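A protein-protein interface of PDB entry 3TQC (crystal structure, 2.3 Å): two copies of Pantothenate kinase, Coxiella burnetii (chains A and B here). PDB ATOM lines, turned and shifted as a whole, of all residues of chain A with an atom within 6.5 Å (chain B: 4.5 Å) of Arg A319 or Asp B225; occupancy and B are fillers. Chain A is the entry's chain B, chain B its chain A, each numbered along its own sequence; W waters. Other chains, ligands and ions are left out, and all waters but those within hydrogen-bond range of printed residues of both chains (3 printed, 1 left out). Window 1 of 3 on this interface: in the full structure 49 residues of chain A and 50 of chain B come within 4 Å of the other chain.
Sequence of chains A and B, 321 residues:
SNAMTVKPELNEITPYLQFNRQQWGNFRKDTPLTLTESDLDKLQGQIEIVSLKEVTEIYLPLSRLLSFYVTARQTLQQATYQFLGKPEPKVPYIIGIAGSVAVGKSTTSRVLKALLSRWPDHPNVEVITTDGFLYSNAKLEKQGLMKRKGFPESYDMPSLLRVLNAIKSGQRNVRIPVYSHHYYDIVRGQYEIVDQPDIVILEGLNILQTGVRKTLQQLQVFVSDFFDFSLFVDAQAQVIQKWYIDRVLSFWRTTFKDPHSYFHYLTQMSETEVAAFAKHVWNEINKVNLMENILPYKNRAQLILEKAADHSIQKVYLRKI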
ATOM      1  N   PRO A  15      22.605  27.278  -7.045  1.00  0.00           N
ATOM      2  CA  PRO A  15      22.000  28.071  -5.987  1.00  0.00           C
ATOM      3  C   PRO A  15      21.503  27.225  -4.822  1.00  0.00           C
ATOM      4  O   PRO A  15      20.842  27.745  -3.925  1.00  0.00           O
ATOM      5  CB  PRO A  15      20.838  28.765  -6.705  1.00  0.00           C
ATOM      6  CG  PRO A  15      20.436  27.768  -7.757  1.00  0.00           C
ATOM      7  CD  PRO A  15      21.735  27.200  -8.242  1.00  0.00           C
ATOM      8  N   TYR A  16      21.828  25.941  -4.837  1.00  0.00           N
ATOM      9  CA  TYR A  16      21.427  25.021  -3.785  1.00  0.00           C
ATOM     10  C   TYR A  16      22.604  24.403  -3.054  1.00  0.00           C
ATOM     11  O   TYR A  16      23.571  23.957  -3.680  1.00  0.00           O
ATOM     12  CB  TYR A  16      20.636  23.862  -4.377  1.00  0.00           C
ATOM     13  CG  TYR A  16      19.306  24.229  -4.929  1.00  0.00           C
ATOM     14  CD1 TYR A  16      18.186  24.235  -4.122  1.00  0.00           C
ATOM     15  CD2 TYR A  16      19.162  24.563  -6.269  1.00  0.00           C
ATOM     16  CE1 TYR A  16      16.959  24.562  -4.628  1.00  0.00           C
ATOM     17  CE2 TYR A  16      17.937  24.889  -6.788  1.00  0.00           C
ATOM     18  CZ  TYR A  16      16.840  24.890  -5.966  1.00  0.00           C
ATOM     19  OH  TYR A  16      15.613  25.210  -6.476  1.00  0.00           O
ATOM     20  N   LEU A  17      22.494  24.366  -1.725  1.00  0.00           N
ATOM     21  CA  LEU A  17      23.258  23.436  -0.911  1.00  0.00           C
ATOM     22  C   LEU A  17      22.708  22.071  -1.237  1.00  0.00           C
ATOM     23  O   LEU A  17      21.503  21.897  -1.359  1.00  0.00           O
ATOM     24  CB  LEU A  17      23.060  23.668   0.595  1.00  0.00           C
ATOM     25  CG  LEU A  17      23.482  24.997   1.188  1.00  0.00           C
ATOM     26  CD1 LEU A  17      23.172  25.011   2.693  1.00  0.00           C
ATOM     27  CD2 LEU A  17      24.957  25.293   0.899  1.00  0.00           C
ATOM     28  N   TYR A  69      13.785  28.756  10.266  1.00  0.00           N
ATOM     29  CA  TYR A  69      13.150  29.735   9.384  1.00  0.00           C
ATOM     30  C   TYR A  69      11.937  30.356  10.037  1.00  0.00           C
ATOM     31  O   TYR A  69      11.755  31.558   9.967  1.00  0.00           O
ATOM     32  CB  TYR A  69      12.740  29.118   8.038  1.00  0.00           C
ATOM     33  CG  TYR A  69      13.887  28.960   7.083  1.00  0.00           C
ATOM     34  CD1 TYR A  69      14.024  29.796   5.988  1.00  0.00           C
ATOM     35  CD2 TYR A  69      14.846  27.966   7.273  1.00  0.00           C
ATOM     36  CE1 TYR A  69      15.095  29.652   5.102  1.00  0.00           C
ATOM     37  CE2 TYR A  69      15.912  27.812   6.392  1.00  0.00           C
ATOM     38  CZ  TYR A  69      16.037  28.669   5.318  1.00  0.00           C
ATOM     39  OH  TYR A  69      17.101  28.526   4.447  1.00  0.00           O
ATOM     40  N   SER A 224       2.606  31.206  -4.457  1.00  0.00           N
ATOM     41  CA  SER A 224       3.911  31.444  -3.848  1.00  0.00           C
ATOM     42  C   SER A 224       4.065  32.833  -3.206  1.00  0.00           C
ATOM     43  O   SER A 224       4.901  33.025  -2.312  1.00  0.00           O
ATOM     44  CB  SER A 224       5.024  31.223  -4.873  1.00  0.00           C
ATOM     45  OG  SER A 224       5.020  32.245  -5.847  1.00  0.00           O
ATOM     46  N   ASN A 299      12.172  23.980  -9.755  1.00  0.00           N
ATOM     47  CA  ASN A 299      13.307  24.786  -9.350  1.00  0.00           C
ATOM     48  C   ASN A 299      12.888  26.080  -8.671  1.00  0.00           C
ATOM     49  O   ASN A 299      13.738  26.874  -8.290  1.00  0.00           O
ATOM     50  CB  ASN A 299      14.240  25.026 -10.538  1.00  0.00           C
ATOM     51  CG  ASN A 299      14.930  23.740 -10.996  1.00  0.00           C
ATOM     52  OD1 ASN A 299      15.024  22.769 -10.237  1.00  0.00           O
ATOM     53  ND2 ASN A 299      15.407  23.724 -12.235  1.00  0.00           N
ATOM     54  N   ARG A 300      11.589  26.296  -8.495  1.00  0.00           N
ATOM     55  CA  ARG A 300      11.143  27.443  -7.703  1.00  0.00           C
ATOM     56  C   ARG A 300      11.182  27.150  -6.203  1.00  0.00           C
ATOM     57  O   ARG A 300      11.082  28.053  -5.419  1.00  0.00           O
ATOM     58  CB  ARG A 300       9.738  27.890  -8.095  1.00  0.00           C
ATOM     59  CG  ARG A 300       9.596  28.353  -9.518  1.00  0.00           C
ATOM     60  CD  ARG A 300       8.286  29.098  -9.693  1.00  0.00           C
ATOM     61  NE  ARG A 300       8.246  30.282  -8.834  1.00  0.00           N
ATOM     62  CZ  ARG A 300       7.179  30.720  -8.170  1.00  0.00           C
ATOM     63  NH1 ARG A 300       6.011  30.092  -8.254  1.00  0.00           N
ATOM     64  NH2 ARG A 300       7.299  31.804  -7.396  1.00  0.00           N
ATOM     65  N   ALA A 301      11.303  25.881  -5.833  1.00  0.00           N
ATOM     66  CA  ALA A 301      11.294  25.441  -4.450  1.00  0.00           C
ATOM     67  C   ALA A 301      12.564  25.818  -3.749  1.00  0.00           C
ATOM     68  O   ALA A 301      13.630  25.848  -4.359  1.00  0.00           O
ATOM     69  CB  ALA A 301      11.117  23.930  -4.381  1.00  0.00           C
ATOM     70  N   GLN A 302      12.447  26.106  -2.461  1.00  0.00           N
ATOM     71  CA  GLN A 302      13.611  26.385  -1.617  1.00  0.00           C
ATOM     72  C   GLN A 302      14.342  25.078  -1.284  1.00  0.00           C
ATOM     73  O   GLN A 302      15.551  25.049  -1.152  1.00  0.00           O
ATOM     74  CB  GLN A 302      13.195  27.066  -0.316  1.00  0.00           C
ATOM     75  CG  GLN A 302      13.049  28.552  -0.385  1.00  0.00           C
ATOM     76  CD  GLN A 302      11.811  28.964  -1.114  1.00  0.00           C
ATOM     77  OE1 GLN A 302      10.717  28.478  -0.826  1.00  0.00           O
ATOM     78  NE2 GLN A 302      11.972  29.852  -2.092  1.00  0.00           N
ATOM     79  N   LEU A 303      13.578  24.010  -1.140  1.00  0.00           N
ATOM     80  CA  LEU A 303      14.115  22.738  -0.716  1.00  0.00           C
ATOM     81  C   LEU A 303      13.549  21.643  -1.606  1.00  0.00           C
ATOM     82  O   LEU A 303      12.345  21.581  -1.842  1.00  0.00           O
ATOM     83  CB  LEU A 303      13.726  22.499   0.740  1.00  0.00           C
ATOM     84  CG  LEU A 303      14.368  21.348   1.500  1.00  0.00           C
ATOM     85  CD1 LEU A 303      14.409  21.702   2.979  1.00  0.00           C
ATOM     86  CD2 LEU A 303      13.594  20.073   1.287  1.00  0.00           C
ATOM     87  N   ILE A 304      14.413  20.797  -2.133  1.00  0.00           N
ATOM     88  CA  ILE A 304      13.941  19.664  -2.901  1.00  0.00           C
ATOM     89  C   ILE A 304      14.361  18.407  -2.187  1.00  0.00           C
ATOM     90  O   ILE A 304      15.527  18.233  -1.872  1.00  0.00           O
ATOM     91  CB  ILE A 304      14.469  19.693  -4.333  1.00  0.00           C
ATOM     92  CG1 ILE A 304      13.983  20.970  -5.033  1.00  0.00           C
ATOM     93  CG2 ILE A 304      14.010  18.458  -5.102  1.00  0.00           C
ATOM     94  CD1 ILE A 304      14.772  21.309  -6.264  1.00  0.00           C
ATOM     95  N   TYR A 317      18.177  19.244  -1.613  1.00  0.00           N
ATOM     96  CA  TYR A 317      18.677  20.509  -2.133  1.00  0.00           C
ATOM     97  C   TYR A 317      18.073  21.604  -1.282  1.00  0.00           C
ATOM     98  O   TYR A 317      16.885  21.586  -1.010  1.00  0.00           O
ATOM     99  CB  TYR A 317      18.245  20.719  -3.573  1.00  0.00           C
ATOM    100  CG  TYR A 317      18.829  19.750  -4.568  1.00  0.00           C
ATOM    101  CD1 TYR A 317      19.973  20.068  -5.279  1.00  0.00           C
ATOM    102  CD2 TYR A 317      18.222  18.521  -4.822  1.00  0.00           C
ATOM    103  CE1 TYR A 317      20.504  19.193  -6.205  1.00  0.00           C
ATOM    104  CE2 TYR A 317      18.750  17.641  -5.756  1.00  0.00           C
ATOM    105  CZ  TYR A 317      19.893  17.982  -6.436  1.00  0.00           C
ATOM    106  OH  TYR A 317      20.435  17.112  -7.362  1.00  0.00           O
ATOM    107  N   LEU A 318      18.882  22.558  -0.851  1.00  0.00           N
ATOM    108  CA  LEU A 318      18.370  23.674  -0.079  1.00  0.00           C
ATOM    109  C   LEU A 318      18.975  24.935  -0.670  1.00  0.00           C
ATOM    110  O   LEU A 318      20.206  25.044  -0.813  1.00  0.00           O
ATOM    111  CB  LEU A 318      18.748  23.519   1.407  1.00  0.00           C
ATOM    112  CG  LEU A 318      18.392  24.658   2.379  1.00  0.00           C
ATOM    113  CD1 LEU A 318      16.899  24.911   2.493  1.00  0.00           C
ATOM    114  CD2 LEU A 318      18.960  24.332   3.747  1.00  0.00           C
ATOM    115  N   ARG A 319      18.121  25.882  -1.025  1.00  0.00           N
ATOM    116  CA  ARG A 319      18.590  27.148  -1.577  1.00  0.00           C
ATOM    117  C   ARG A 319      19.610  27.809  -0.656  1.00  0.00           C
ATOM    118  O   ARG A 319      19.420  27.883   0.574  1.00  0.00           O
ATOM    119  CB  ARG A 319      17.433  28.112  -1.830  1.00  0.00           C
ATOM    120  CG  ARG A 319      16.652  27.857  -3.129  1.00  0.00           C
ATOM    121  CD  ARG A 319      17.483  28.126  -4.386  1.00  0.00           C
ATOM    122  NE  ARG A 319      18.058  29.472  -4.367  1.00  0.00           N
ATOM    123  CZ  ARG A 319      17.426  30.591  -4.730  1.00  0.00           C
ATOM    124  NH1 ARG A 319      16.190  30.555  -5.190  1.00  0.00           N
ATOM    125  NH2 ARG A 319      18.055  31.764  -4.638  1.00  0.00           N
ATOM    126  N   LYS A 320      20.704  28.280  -1.245  1.00  0.00           N
ATOM    127  CA  LYS A 320      21.707  28.984  -0.460  1.00  0.00           C
ATOM    128  C   LYS A 320      21.127  30.309   0.006  1.00  0.00           C
ATOM    129  O   LYS A 320      20.381  30.952  -0.721  1.00  0.00           O
ATOM    130  CB  LYS A 320      22.959  29.229  -1.270  1.00  0.00           C
ATOM    131  CG  LYS A 320      23.622  27.966  -1.772  1.00  0.00           C
ATOM    132  CD  LYS A 320      24.820  28.298  -2.643  1.00  0.00           C
ATOM    133  CE  LYS A 320      25.557  27.048  -3.100  1.00  0.00           C
ATOM    134  NZ  LYS A 320      26.572  27.321  -4.155  1.00  0.00           N
ATOM    135  N   ILE A 321      21.460  30.704   1.223  1.00  0.00           N
ATOM    136  CA  ILE A 321      21.032  31.987   1.737  1.00  0.00           C
ATOM    137  C   ILE A 321      22.245  32.745   2.239  1.00  0.00           C
ATOM    138  O   ILE A 321      23.403  32.279   2.128  1.00  0.00           O
ATOM    139  CB  ILE A 321      19.948  31.854   2.847  1.00  0.00           C
ATOM    140  CG1 ILE A 321      20.430  31.037   4.049  1.00  0.00           C
ATOM    141  CG2 ILE A 321      18.715  31.187   2.316  1.00  0.00           C
ATOM    142  CD1 ILE A 321      19.567  31.307   5.319  1.00  0.00           C
ATOM    143  OXT ILE A 321      22.098  33.855   2.748  1.00  0.00           O
ATOM    144  N   LYS B 168      23.397  34.161  -6.812  1.00  0.00           N
ATOM    145  CA  LYS B 168      22.755  33.388  -5.763  1.00  0.00           C
ATOM    146  C   LYS B 168      23.373  32.010  -5.569  1.00  0.00           C
ATOM    147  O   LYS B 168      22.962  31.263  -4.674  1.00  0.00           O
ATOM    148  CB  LYS B 168      21.251  33.266  -6.044  1.00  0.00           C
ATOM    149  CG  LYS B 168      20.464  34.493  -5.581  1.00  0.00           C
ATOM    150  CD  LYS B 168      20.446  34.607  -4.066  1.00  0.00           C
ATOM    151  CE  LYS B 168      19.404  35.611  -3.581  1.00  0.00           C
ATOM    152  NZ  LYS B 168      19.394  35.714  -2.093  1.00  0.00           N
ATOM    153  N   VAL B 221      11.654  29.416 -13.974  1.00  0.00           N
ATOM    154  CA  VAL B 221      11.952  30.177 -12.780  1.00  0.00           C
ATOM    155  C   VAL B 221      11.830  31.623 -13.154  1.00  0.00           C
ATOM    156  O   VAL B 221      11.982  31.999 -14.310  1.00  0.00           O
ATOM    157  CB  VAL B 221      13.370  29.926 -12.253  1.00  0.00           C
ATOM    158  CG1 VAL B 221      13.511  28.467 -11.809  1.00  0.00           C
ATOM    159  CG2 VAL B 221      14.400  30.288 -13.331  1.00  0.00           C
ATOM    160  N   PHE B 222      11.550  32.433 -12.161  1.00  0.00           N
ATOM    161  CA  PHE B 222      11.292  33.821 -12.385  1.00  0.00           C
ATOM    162  C   PHE B 222      12.382  34.616 -11.702  1.00  0.00           C
ATOM    163  O   PHE B 222      13.074  34.111 -10.808  1.00  0.00           O
ATOM    164  CB  PHE B 222       9.938  34.179 -11.795  1.00  0.00           C
ATOM    165  CG  PHE B 222       8.854  33.197 -12.114  1.00  0.00           C
ATOM    166  CD1 PHE B 222       8.696  32.710 -13.398  1.00  0.00           C
ATOM    167  CD2 PHE B 222       7.953  32.806 -11.139  1.00  0.00           C
ATOM    168  CE1 PHE B 222       7.674  31.826 -13.693  1.00  0.00           C
ATOM    169  CE2 PHE B 222       6.949  31.934 -11.425  1.00  0.00           C
ATOM    170  CZ  PHE B 222       6.804  31.438 -12.697  1.00  0.00           C
ATOM    171  N   VAL B 223      12.495  35.872 -12.096  1.00  0.00           N
ATOM    172  CA  VAL B 223      13.420  36.776 -11.445  1.00  0.00           C
ATOM    173  C   VAL B 223      13.222  36.791  -9.929  1.00  0.00           C
ATOM    174  O   VAL B 223      14.204  36.781  -9.174  1.00  0.00           O
ATOM    175  CB  VAL B 223      13.298  38.194 -11.999  1.00  0.00           C
ATOM    176  CG1 VAL B 223      14.255  39.143 -11.230  1.00  0.00           C
ATOM    177  CG2 VAL B 223      13.575  38.188 -13.505  1.00  0.00           C
ATOM    178  N   SER B 224      11.960  36.780  -9.494  1.00  0.00           N
ATOM    179  CA  SER B 224      11.630  36.776  -8.059  1.00  0.00           C
ATOM    180  C   SER B 224      12.161  35.578  -7.287  1.00  0.00           C
ATOM    181  O   SER B 224      12.392  35.670  -6.083  1.00  0.00           O
ATOM    182  CB  SER B 224      10.114  36.903  -7.832  1.00  0.00           C
ATOM    183  OG  SER B 224       9.421  35.724  -8.205  1.00  0.00           O
ATOM    184  N   ASP B 225      12.389  34.463  -7.963  1.00  0.00           N
ATOM    185  CA  ASP B 225      12.982  33.308  -7.294  1.00  0.00           C
ATOM    186  C   ASP B 225      14.444  33.567  -6.884  1.00  0.00           C
ATOM    187  O   ASP B 225      15.037  32.765  -6.144  1.00  0.00           O
ATOM    188  CB  ASP B 225      12.892  32.081  -8.193  1.00  0.00           C
ATOM    189  CG  ASP B 225      11.449  31.683  -8.483  1.00  0.00           C
ATOM    190  OD1 ASP B 225      11.140  31.286  -9.618  1.00  0.00           O
ATOM    191  OD2 ASP B 225      10.603  31.792  -7.578  1.00  0.00           O
ATOM    192  N   PHE B 226      15.018  34.673  -7.368  1.00  0.00           N
ATOM    193  CA  PHE B 226      16.383  35.033  -7.062  1.00  0.00           C
ATOM    194  C   PHE B 226      16.513  36.276  -6.218  1.00  0.00           C
ATOM    195  O   PHE B 226      17.625  36.763  -6.007  1.00  0.00           O
ATOM    196  CB  PHE B 226      17.179  35.210  -8.339  1.00  0.00           C
ATOM    197  CG  PHE B 226      17.360  33.942  -9.089  1.00  0.00           C
ATOM    198  CD1 PHE B 226      16.741  33.750 -10.317  1.00  0.00           C
ATOM    199  CD2 PHE B 226      18.113  32.920  -8.544  1.00  0.00           C
ATOM    200  CE1 PHE B 226      16.887  32.577 -10.984  1.00  0.00           C
ATOM    201  CE2 PHE B 226      18.268  31.732  -9.212  1.00  0.00           C
ATOM    202  CZ  PHE B 226      17.650  31.557 -10.435  1.00  0.00           C
ATOM    203  N   PHE B 227      15.413  36.805  -5.725  1.00  0.00           N
ATOM    204  CA  PHE B 227      15.515  37.882  -4.768  1.00  0.00           C
ATOM    205  C   PHE B 227      14.716  37.616  -3.506  1.00  0.00           C
ATOM    206  O   PHE B 227      13.904  36.706  -3.432  1.00  0.00           O
ATOM    207  CB  PHE B 227      15.224  39.252  -5.404  1.00  0.00           C
ATOM    208  CG  PHE B 227      13.821  39.446  -5.922  1.00  0.00           C
ATOM    209  CD1 PHE B 227      12.713  39.341  -5.084  1.00  0.00           C
ATOM    210  CD2 PHE B 227      13.618  39.843  -7.238  1.00  0.00           C
ATOM    211  CE1 PHE B 227      11.423  39.579  -5.565  1.00  0.00           C
ATOM    212  CE2 PHE B 227      12.350  40.093  -7.719  1.00  0.00           C
ATOM    213  CZ  PHE B 227      11.245  39.956  -6.883  1.00  0.00           C
HETATM  214  O   HOH W   1      16.288  34.320  -3.410  1.00  0.00           O
HETATM  215  O   HOH W   2       9.539  33.754  -6.671  1.00  0.00           O
HETATM  216  O   HOH W   3      18.801  33.184  -1.097  1.00  0.00           O
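The side-chain carboxylate (OD2) of Asp B225 lies within salt-bridge range of the guanidinium group (NE) of Arg A300 (3.1 Å).
The backbone carbonyl oxygen (O) of Asp B225 is in hydrogen-bond range of the guanidinium group (NH1) of Arg A319.
N of Phe B222 lies within hydrogen-bond range of OD1 of Asp B225, 2.8 Å away.
The guanidinium group (NE) of Arg A319 sits at hydrogen-bond distance from the backbone carbonyl oxygen (O) of Pro A15, at 3.3 Å.
The backbone NH of Lys A320 is in hydrogen-bond range of the backbone carbonyl oxygen of Pro A15.
The backbone carbonyl oxygen of Asn A299 lies within hydrogen-bond range of the side-chain hydroxyl of Tyr A16, 3.1 Å away.
The side-chain hydroxyl (OG) of Ser A224 lies within hydrogen-bond range of the guanidinium group (NH2) of Arg A300 (2.8 Å).
The backbone NH (N) of Arg A319 is in hydrogen-bond range of the backbone carbonyl oxygen (O) of Gln A302 (2.7 Å).
Lys B168 touches Pro A15.
Asn A299 touches Val B221 (CB to CG1, 3.7 Å).
Arg A300 touches Phe B222 (NE to CE2, 3.3 Å).
NH2 of Arg A319 touches CD of Lys B168, at 3.8 Å.
CB of Lys A320 touches O of Lys B168 (3.97 Å).
Of the printed residues of chain B, Pro A15 touches Lys B168.
Of the printed residues of chain B, Asn A299 touches Val B221 (3.7 Å).
Printed residues of chain B within 4 Å of Arg A319: Lys B168 and Asp B225.
Of the printed residues of chain B, Lys A320 touches Lys B168 (3.97 Å).
Of the printed residues of chain A, Lys B168 touches Pro A15 (3.6 Å), Arg A319 (3.8 Å) and Lys A320 (3.97 Å).
Of the printed residues of chain A, Val B221 touches Asn A299.
Printed residues of chain A within 4 Å of Asp B225: Arg A300 and Arg A319.
Phe B227 touches none of the printed residues of chain A.
The nearest printed residue of chain B that does not touch Asn A299 is Asp B225 (5.3 Å).
Hydrophobic or aromatic side chains of chain B that line the printed part of chain A: Val B221 and Phe B222.
Along chain B the printed residues that touch a printed residue of chain A span positions 168 to 225.
Of the 16 printed residues of chain A, 5 touch a printed residue of chain B.
Printed residues of chain A that touch a printed residue of chain B: Pro A15, Asn A299, Arg A300, Arg A319 and Lys A320.
Among the printed residues, 7 pairs touch across the chains.
1 position is printed for both chains.
Of the 7 pairs that touch across the chains among the printed residues, none has its exchanged pair printed and touching as well.
Water W2 lies within hydrogen-bond range of OD2 of Asp B225, OG of Ser B224 and NH2 of Arg A300.
Water W3 lies within hydrogen-bond range of the backbone carbonyl oxygen of Lys A320 and the side-chain amino group of Lys B168.
Water W1 lies within hydrogen-bond range of NH2 of Arg A319 (3.3 Å), O of Phe B227 (3.4 Å) and O of Asp B225 (3.4 Å).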
